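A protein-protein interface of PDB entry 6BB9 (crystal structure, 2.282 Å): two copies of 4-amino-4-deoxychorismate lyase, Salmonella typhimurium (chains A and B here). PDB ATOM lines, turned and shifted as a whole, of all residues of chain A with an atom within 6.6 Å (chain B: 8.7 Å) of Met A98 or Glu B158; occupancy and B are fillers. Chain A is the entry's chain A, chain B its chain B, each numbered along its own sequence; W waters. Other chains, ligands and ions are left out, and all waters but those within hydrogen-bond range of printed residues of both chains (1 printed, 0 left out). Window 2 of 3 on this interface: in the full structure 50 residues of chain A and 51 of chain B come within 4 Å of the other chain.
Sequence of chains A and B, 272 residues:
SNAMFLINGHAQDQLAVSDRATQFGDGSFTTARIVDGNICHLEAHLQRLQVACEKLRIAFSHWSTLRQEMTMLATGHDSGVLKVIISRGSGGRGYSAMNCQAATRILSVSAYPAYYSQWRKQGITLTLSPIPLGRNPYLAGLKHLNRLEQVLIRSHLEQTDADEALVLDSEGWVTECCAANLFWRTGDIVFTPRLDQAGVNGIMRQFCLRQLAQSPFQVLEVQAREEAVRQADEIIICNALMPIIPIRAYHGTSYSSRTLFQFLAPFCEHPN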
ATOM      1  N   ARG A  20      30.096  10.864 -28.329  1.00  0.00           N
ATOM      2  CA  ARG A  20      30.257   9.620 -27.586  1.00  0.00           C
ATOM      3  C   ARG A  20      31.330   8.721 -28.179  1.00  0.00           C
ATOM      4  O   ARG A  20      31.696   7.730 -27.545  1.00  0.00           O
ATOM      5  CB  ARG A  20      28.915   8.895 -27.489  1.00  0.00           C
ATOM      6  CG  ARG A  20      27.904   9.625 -26.607  1.00  0.00           C
ATOM      7  CD  ARG A  20      26.490   9.098 -26.797  1.00  0.00           C
ATOM      8  NE  ARG A  20      26.358   7.696 -26.413  1.00  0.00           N
ATOM      9  CZ  ARG A  20      25.883   7.281 -25.241  1.00  0.00           C
ATOM     10  NH1 ARG A  20      25.488   8.157 -24.326  1.00  0.00           N
ATOM     11  NH2 ARG A  20      25.795   5.985 -24.989  1.00  0.00           N
ATOM     12  N   GLY A  91      25.152  13.453 -26.362  1.00  0.00           N
ATOM     13  CA  GLY A  91      23.952  13.431 -25.555  1.00  0.00           C
ATOM     14  C   GLY A  91      23.858  12.177 -24.709  1.00  0.00           C
ATOM     15  O   GLY A  91      24.798  11.388 -24.596  1.00  0.00           O
ATOM     16  N   GLY A  92      22.690  12.004 -24.108  1.00  0.00           N
ATOM     17  CA  GLY A  92      22.458  10.903 -23.206  1.00  0.00           C
ATOM     18  C   GLY A  92      22.972  11.188 -21.806  1.00  0.00           C
ATOM     19  O   GLY A  92      23.794  12.074 -21.571  1.00  0.00           O
ATOM     20  N   ARG A  93      22.461  10.410 -20.860  1.00  0.00           N
ATOM     21  CA  ARG A  93      22.820  10.530 -19.451  1.00  0.00           C
ATOM     22  C   ARG A  93      23.707   9.340 -19.104  1.00  0.00           C
ATOM     23  O   ARG A  93      23.227   8.213 -18.963  1.00  0.00           O
ATOM     24  CB  ARG A  93      21.573  10.576 -18.578  1.00  0.00           C
ATOM     25  CG  ARG A  93      20.548  11.618 -18.990  1.00  0.00           C
ATOM     26  CD  ARG A  93      20.641  12.851 -18.113  1.00  0.00           C
ATOM     27  NE  ARG A  93      19.399  13.618 -18.122  1.00  0.00           N
ATOM     28  CZ  ARG A  93      19.118  14.600 -17.268  1.00  0.00           C
ATOM     29  NH1 ARG A  93      17.961  15.240 -17.348  1.00  0.00           N
ATOM     30  NH2 ARG A  93      19.993  14.937 -16.327  1.00  0.00           N
ATOM     31  N   TYR A  95      25.919   6.264 -19.542  1.00  0.00           N
ATOM     32  CA  TYR A  95      25.976   5.254 -20.587  1.00  0.00           C
ATOM     33  C   TYR A  95      24.699   5.215 -21.410  1.00  0.00           C
ATOM     34  O   TYR A  95      24.728   4.757 -22.559  1.00  0.00           O
ATOM     35  CB  TYR A  95      26.239   3.884 -19.971  1.00  0.00           C
ATOM     36  CG  TYR A  95      27.596   3.739 -19.329  1.00  0.00           C
ATOM     37  CD1 TYR A  95      28.758   4.079 -20.019  1.00  0.00           C
ATOM     38  CD2 TYR A  95      27.720   3.257 -18.027  1.00  0.00           C
ATOM     39  CE1 TYR A  95      30.004   3.943 -19.430  1.00  0.00           C
ATOM     40  CE2 TYR A  95      28.957   3.113 -17.433  1.00  0.00           C
ATOM     41  CZ  TYR A  95      30.094   3.451 -18.140  1.00  0.00           C
ATOM     42  OH  TYR A  95      31.324   3.311 -17.541  1.00  0.00           O
ATOM     43  N   SER A  96      23.590   5.686 -20.849  1.00  0.00           N
ATOM     44  CA  SER A  96      22.317   5.683 -21.553  1.00  0.00           C
ATOM     45  C   SER A  96      22.388   6.526 -22.821  1.00  0.00           C
ATOM     46  O   SER A  96      23.099   7.532 -22.890  1.00  0.00           O
ATOM     47  CB  SER A  96      21.206   6.203 -20.639  1.00  0.00           C
ATOM     48  OG  SER A  96      19.957   6.185 -21.305  1.00  0.00           O
ATOM     49  N   ALA A  97      21.632   6.098 -23.833  1.00  0.00           N
ATOM     50  CA  ALA A  97      21.553   6.775 -25.121  1.00  0.00           C
ATOM     51  C   ALA A  97      20.171   7.359 -25.393  1.00  0.00           C
ATOM     52  O   ALA A  97      19.863   7.699 -26.539  1.00  0.00           O
ATOM     53  CB  ALA A  97      21.937   5.818 -26.247  1.00  0.00           C
ATOM     54  N   MET A  98      19.320   7.458 -24.377  1.00  0.00           N
ATOM     55  CA  MET A  98      17.997   8.027 -24.590  1.00  0.00           C
ATOM     56  C   MET A  98      18.116   9.523 -24.826  1.00  0.00           C
ATOM     57  O   MET A  98      18.970  10.190 -24.238  1.00  0.00           O
ATOM     58  CB  MET A  98      17.087   7.745 -23.394  1.00  0.00           C
ATOM     59  CG  MET A  98      16.632   6.292 -23.306  1.00  0.00           C
ATOM     60  SD  MET A  98      15.641   5.954 -21.838  1.00  0.00           S
ATOM     61  CE  MET A  98      14.499   7.336 -21.870  1.00  0.00           C
ATOM     62  N   ASN A  99      17.255  10.047 -25.697  1.00  0.00           N
ATOM     63  CA  ASN A  99      17.283  11.461 -26.065  1.00  0.00           C
ATOM     64  C   ASN A  99      18.683  11.847 -26.533  1.00  0.00           C
ATOM     65  O   ASN A  99      19.276  12.832 -26.088  1.00  0.00           O
ATOM     66  CB  ASN A  99      16.815  12.343 -24.904  1.00  0.00           C
ATOM     67  N   CYS A 100      19.224  11.027 -27.425  1.00  0.00           N
ATOM     68  CA  CYS A 100      20.558  11.225 -27.961  1.00  0.00           C
ATOM     69  C   CYS A 100      20.476  11.976 -29.280  1.00  0.00           C
ATOM     70  O   CYS A 100      19.668  11.643 -30.152  1.00  0.00           O
ATOM     71  CB  CYS A 100      21.270   9.891 -28.171  1.00  0.00           C
ATOM     72  SG  CYS A 100      23.022   9.950 -27.796  1.00  0.00           S
ATOM     73  N   GLN A 101      21.329  12.986 -29.421  1.00  0.00           N
ATOM     74  CA  GLN A 101      21.324  13.817 -30.612  1.00  0.00           C
ATOM     75  C   GLN A 101      21.800  13.010 -31.825  1.00  0.00           C
ATOM     76  O   GLN A 101      22.207  11.848 -31.721  1.00  0.00           O
ATOM     77  CB  GLN A 101      22.188  15.061 -30.394  1.00  0.00           C
ATOM     78  N   THR B 127      17.825  -6.697 -12.773  1.00  0.00           N
ATOM     79  CA  THR B 127      17.487  -7.656 -13.808  1.00  0.00           C
ATOM     80  C   THR B 127      18.781  -8.188 -14.407  1.00  0.00           C
ATOM     81  O   THR B 127      19.806  -7.503 -14.409  1.00  0.00           O
ATOM     82  CB  THR B 127      16.595  -7.026 -14.883  1.00  0.00           C
ATOM     83  OG1 THR B 127      15.987  -8.055 -15.672  1.00  0.00           O
ATOM     84  CG2 THR B 127      17.403  -6.102 -15.785  1.00  0.00           C
ATOM     85  N   GLN B 150      28.980  -1.440 -21.755  1.00  0.00           N
ATOM     86  CA  GLN B 150      28.034  -0.790 -20.854  1.00  0.00           C
ATOM     87  C   GLN B 150      26.955  -0.045 -21.630  1.00  0.00           C
ATOM     88  O   GLN B 150      25.795  -0.013 -21.199  1.00  0.00           O
ATOM     89  CB  GLN B 150      28.772   0.152 -19.897  1.00  0.00           C
ATOM     90  CG  GLN B 150      29.558  -0.575 -18.802  1.00  0.00           C
ATOM     91  CD  GLN B 150      30.734  -1.376 -19.342  1.00  0.00           C
ATOM     92  OE1 GLN B 150      31.368  -0.985 -20.324  1.00  0.00           O
ATOM     93  NE2 GLN B 150      31.024  -2.508 -18.710  1.00  0.00           N
ATOM     94  N   VAL B 151      27.306   0.537 -22.782  1.00  0.00           N
ATOM     95  CA  VAL B 151      26.297   1.185 -23.617  1.00  0.00           C
ATOM     96  C   VAL B 151      25.232   0.178 -24.042  1.00  0.00           C
ATOM     97  O   VAL B 151      24.030   0.450 -23.949  1.00  0.00           O
ATOM     98  CB  VAL B 151      26.958   1.869 -24.830  1.00  0.00           C
ATOM     99  CG1 VAL B 151      25.904   2.472 -25.754  1.00  0.00           C
ATOM    100  CG2 VAL B 151      27.923   2.946 -24.360  1.00  0.00           C
ATOM    101  N   LEU B 152      25.650  -1.008 -24.492  1.00  0.00           N
ATOM    102  CA  LEU B 152      24.676  -2.024 -24.881  1.00  0.00           C
ATOM    103  C   LEU B 152      23.895  -2.527 -23.671  1.00  0.00           C
ATOM    104  O   LEU B 152      22.677  -2.714 -23.751  1.00  0.00           O
ATOM    105  CB  LEU B 152      25.373  -3.184 -25.603  1.00  0.00           C
ATOM    106  CG  LEU B 152      26.154  -2.843 -26.883  1.00  0.00           C
ATOM    107  CD1 LEU B 152      26.834  -4.067 -27.475  1.00  0.00           C
ATOM    108  CD2 LEU B 152      25.257  -2.192 -27.922  1.00  0.00           C
ATOM    109  N   ILE B 153      24.575  -2.725 -22.538  1.00  0.00           N
ATOM    110  CA  ILE B 153      23.898  -3.156 -21.313  1.00  0.00           C
ATOM    111  C   ILE B 153      22.819  -2.155 -20.925  1.00  0.00           C
ATOM    112  O   ILE B 153      21.687  -2.529 -20.594  1.00  0.00           O
ATOM    113  CB  ILE B 153      24.912  -3.347 -20.169  1.00  0.00           C
ATOM    114  CG1 ILE B 153      25.787  -4.580 -20.404  1.00  0.00           C
ATOM    115  CG2 ILE B 153      24.192  -3.475 -18.817  1.00  0.00           C
ATOM    116  CD1 ILE B 153      27.121  -4.522 -19.675  1.00  0.00           C
ATOM    117  N   ARG B 154      23.152  -0.864 -20.957  1.00  0.00           N
ATOM    118  CA  ARG B 154      22.152   0.143 -20.616  1.00  0.00           C
ATOM    119  C   ARG B 154      21.003   0.127 -21.617  1.00  0.00           C
ATOM    120  O   ARG B 154      19.835   0.260 -21.235  1.00  0.00           O
ATOM    121  CB  ARG B 154      22.804   1.523 -20.549  1.00  0.00           C
ATOM    122  CG  ARG B 154      21.884   2.608 -20.055  1.00  0.00           C
ATOM    123  CD  ARG B 154      21.358   2.302 -18.676  1.00  0.00           C
ATOM    124  NE  ARG B 154      20.159   3.081 -18.394  1.00  0.00           N
ATOM    125  CZ  ARG B 154      19.586   3.154 -17.200  1.00  0.00           C
ATOM    126  NH1 ARG B 154      20.113   2.494 -16.176  1.00  0.00           N
ATOM    127  NH2 ARG B 154      18.491   3.885 -17.031  1.00  0.00           N
ATOM    128  N   SER B 155      21.316  -0.077 -22.900  1.00  0.00           N
ATOM    129  CA  SER B 155      20.283  -0.124 -23.930  1.00  0.00           C
ATOM    130  C   SER B 155      19.323  -1.291 -23.704  1.00  0.00           C
ATOM    131  O   SER B 155      18.100  -1.128 -23.808  1.00  0.00           O
ATOM    132  CB  SER B 155      20.939  -0.207 -25.311  1.00  0.00           C
ATOM    133  OG  SER B 155      20.015   0.030 -26.357  1.00  0.00           O
ATOM    134  N   HIS B 156      19.848  -2.477 -23.388  1.00  0.00           N
ATOM    135  CA  HIS B 156      18.956  -3.606 -23.152  1.00  0.00           C
ATOM    136  C   HIS B 156      18.190  -3.445 -21.842  1.00  0.00           C
ATOM    137  O   HIS B 156      17.018  -3.827 -21.759  1.00  0.00           O
ATOM    138  CB  HIS B 156      19.753  -4.912 -23.189  1.00  0.00           C
ATOM    139  CG  HIS B 156      20.056  -5.380 -24.579  1.00  0.00           C
ATOM    140  ND1 HIS B 156      21.022  -4.791 -25.371  1.00  0.00           N
ATOM    141  CD2 HIS B 156      19.500  -6.359 -25.333  1.00  0.00           C
ATOM    142  CE1 HIS B 156      21.055  -5.394 -26.546  1.00  0.00           C
ATOM    143  NE2 HIS B 156      20.145  -6.353 -26.548  1.00  0.00           N
ATOM    144  N   LEU B 157      18.821  -2.844 -20.831  1.00  0.00           N
ATOM    145  CA  LEU B 157      18.159  -2.596 -19.554  1.00  0.00           C
ATOM    146  C   LEU B 157      16.950  -1.680 -19.719  1.00  0.00           C
ATOM    147  O   LEU B 157      15.928  -1.857 -19.040  1.00  0.00           O
ATOM    148  CB  LEU B 157      19.167  -1.993 -18.577  1.00  0.00           C
ATOM    149  CG  LEU B 157      18.693  -1.449 -17.234  1.00  0.00           C
ATOM    150  CD1 LEU B 157      18.121  -2.576 -16.389  1.00  0.00           C
ATOM    151  CD2 LEU B 157      19.837  -0.754 -16.508  1.00  0.00           C
ATOM    152  N   GLU B 158      17.049  -0.693 -20.617  1.00  0.00           N
ATOM    153  CA  GLU B 158      15.971   0.268 -20.820  1.00  0.00           C
ATOM    154  C   GLU B 158      14.739  -0.359 -21.453  1.00  0.00           C
ATOM    155  O   GLU B 158      13.662   0.245 -21.407  1.00  0.00           O
ATOM    156  CB  GLU B 158      16.457   1.434 -21.690  1.00  0.00           C
ATOM    157  CG  GLU B 158      17.406   2.373 -20.973  1.00  0.00           C
ATOM    158  CD  GLU B 158      18.161   3.296 -21.910  1.00  0.00           C
ATOM    159  OE1 GLU B 158      18.116   3.091 -23.144  1.00  0.00           O
ATOM    160  OE2 GLU B 158      18.808   4.230 -21.399  1.00  0.00           O
ATOM    161  N   GLN B 159      14.870  -1.542 -22.051  1.00  0.00           N
ATOM    162  CA  GLN B 159      13.713  -2.271 -22.551  1.00  0.00           C
ATOM    163  C   GLN B 159      12.926  -2.960 -21.443  1.00  0.00           C
ATOM    164  O   GLN B 159      11.937  -3.634 -21.742  1.00  0.00           O
ATOM    165  CB  GLN B 159      14.141  -3.324 -23.577  1.00  0.00           C
ATOM    166  CG  GLN B 159      15.013  -2.808 -24.708  1.00  0.00           C
ATOM    167  CD  GLN B 159      15.559  -3.939 -25.560  1.00  0.00           C
ATOM    168  OE1 GLN B 159      16.708  -3.906 -25.998  1.00  0.00           O
ATOM    169  NE2 GLN B 159      14.737  -4.958 -25.783  1.00  0.00           N
ATOM    170  N   THR B 160      13.342  -2.827 -20.187  1.00  0.00           N
ATOM    171  CA  THR B 160      12.662  -3.470 -19.072  1.00  0.00           C
ATOM    172  C   THR B 160      12.273  -2.421 -18.036  1.00  0.00           C
ATOM    173  O   THR B 160      12.562  -1.227 -18.182  1.00  0.00           O
ATOM    174  CB  THR B 160      13.538  -4.545 -18.421  1.00  0.00           C
ATOM    175  OG1 THR B 160      14.530  -3.918 -17.600  1.00  0.00           O
ATOM    176  CG2 THR B 160      14.226  -5.402 -19.476  1.00  0.00           C
ATOM    177  N   ASP B 161      11.628  -2.894 -16.970  1.00  0.00           N
ATOM    178  CA  ASP B 161      11.186  -2.066 -15.859  1.00  0.00           C
ATOM    179  C   ASP B 161      12.190  -2.024 -14.713  1.00  0.00           C
ATOM    180  O   ASP B 161      11.876  -1.471 -13.655  1.00  0.00           O
ATOM    181  CB  ASP B 161       9.837  -2.567 -15.325  1.00  0.00           C
ATOM    182  CG  ASP B 161       8.647  -2.019 -16.105  1.00  0.00           C
ATOM    183  OD1 ASP B 161       8.839  -1.446 -17.201  1.00  0.00           O
ATOM    184  OD2 ASP B 161       7.508  -2.163 -15.604  1.00  0.00           O
ATOM    185  N   ALA B 162      13.376  -2.594 -14.887  1.00  0.00           N
ATOM    186  CA  ALA B 162      14.357  -2.607 -13.813  1.00  0.00           C
ATOM    187  C   ALA B 162      15.235  -1.362 -13.866  1.00  0.00           C
ATOM    188  O   ALA B 162      15.427  -0.746 -14.916  1.00  0.00           O
ATOM    189  CB  ALA B 162      15.227  -3.864 -13.880  1.00  0.00           C
ATOM    190  N   ASP B 163      15.782  -1.005 -12.705  1.00  0.00           N
ATOM    191  CA  ASP B 163      16.619   0.181 -12.576  1.00  0.00           C
ATOM    192  C   ASP B 163      18.087  -0.082 -12.896  1.00  0.00           C
ATOM    193  O   ASP B 163      18.758   0.789 -13.459  1.00  0.00           O
ATOM    194  CB  ASP B 163      16.479   0.749 -11.165  1.00  0.00           C
ATOM    195  CG  ASP B 163      15.043   1.077 -10.818  1.00  0.00           C
ATOM    196  OD1 ASP B 163      14.377   1.753 -11.635  1.00  0.00           O
ATOM    197  OD2 ASP B 163      14.569   0.635  -9.750  1.00  0.00           O
ATOM    198  N   GLU B 164      18.616  -1.253 -12.536  1.00  0.00           N
ATOM    199  CA  GLU B 164      20.000  -1.588 -12.836  1.00  0.00           C
ATOM    200  C   GLU B 164      20.082  -3.040 -13.278  1.00  0.00           C
ATOM    201  O   GLU B 164      19.154  -3.832 -13.086  1.00  0.00           O
ATOM    202  CB  GLU B 164      20.938  -1.342 -11.639  1.00  0.00           C
ATOM    203  CG  GLU B 164      21.886  -0.131 -11.781  1.00  0.00           C
ATOM    204  CD  GLU B 164      23.066  -0.365 -12.733  1.00  0.00           C
ATOM    205  OE1 GLU B 164      23.091  -1.402 -13.427  1.00  0.00           O
ATOM    206  OE2 GLU B 164      23.975   0.494 -12.787  1.00  0.00           O
ATOM    207  N   ALA B 165      21.219  -3.387 -13.866  1.00  0.00           N
ATOM    208  CA  ALA B 165      21.437  -4.709 -14.427  1.00  0.00           C
ATOM    209  C   ALA B 165      22.479  -5.460 -13.613  1.00  0.00           C
ATOM    210  O   ALA B 165      23.438  -4.863 -13.119  1.00  0.00           O
ATOM    211  CB  ALA B 165      21.886  -4.611 -15.888  1.00  0.00           C
ATOM    212  N   CYS B 178      25.769  -2.406 -14.295  1.00  0.00           N
ATOM    213  CA  CYS B 178      26.025  -1.633 -15.501  1.00  0.00           C
ATOM    214  C   CYS B 178      26.969  -0.470 -15.222  1.00  0.00           C
ATOM    215  O   CYS B 178      27.927  -0.240 -15.969  1.00  0.00           O
ATOM    216  CB  CYS B 178      24.711  -1.124 -16.088  1.00  0.00           C
ATOM    217  SG  CYS B 178      24.934  -0.180 -17.613  1.00  0.00           S
HETATM  218  O   HOH W   1      22.514   3.063 -23.682  1.00  0.00           O
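Met A98 touches just one residue of chain B: Glu B158.
Glu B158 touches just these residues of chain A: Ser A96 (2.3 Å) and Met A98 (3.5 Å).
No residue of chain B comes within 4 Å of Ala A97.
No residue of chain B comes within 4 Å of Asn A99.
Printed residues of chain A within 4 Å of Arg B154: Ser A96.
Printed residues of chain A within 4 Å of Cys B178: Tyr A95.
Of the printed residues of chain A, Gln B150 touches Tyr A95.
No position is printed for both chains.
Of the 6 pairs that touch across the chains among the printed residues, none has its exchanged pair printed and touching as well.
The side-chain carboxylate (OE2) of Glu B158 lies close to the side-chain sulfur (SD) of Met A98.
The side-chain carboxylate (OE2) of Glu B158 sits close to the side-chain hydroxyl (OG) of Ser A96, at 2.3 Å.
Hydrophobic or aromatic side chains of chain B that line the printed part of chain A: Val B151.
Among the printed residues, 6 pairs touch across the chains.
Water W1 lies within hydrogen-bond range of O of Tyr A95, O of Val B151, N of Ala A97 and N of Ser B155.
Among the printed residues, pairs that only touch across the chains: Arg A20 with Val B151 (3.6 Å), Tyr A95 with Gln B150 (3.8 Å), Tyr A95 with Cys B178 (3.8 Å) and Ser A96 with Arg B154 (3.4 Å).
The guanidinium group (NH1) of Arg B154 lies within hydrogen-bond range of the backbone carbonyl oxygen (O) of Asp B163, at 3.5 Å.
NH1 of Arg A20 sits at hydrogen-bond distance from O of Gly A91 (3.3 Å).
The guanidinium group of Arg B154 lies within salt-bridge range of the side-chain carboxylate of Glu B158 (3.5 Å).
OG of Ser A96 lies within hydrogen-bond range of N of Met A98 (3.4 Å).
The side-chain sulfur of Cys B178 lies within hydrogen-bond range of the backbone carbonyl oxygen of Gln B150, at 3.7 Å.
The guanidinium group of Arg A20 sits at hydrogen-bond distance from the backbone carbonyl oxygen of Ser A96 (2.9 Å).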
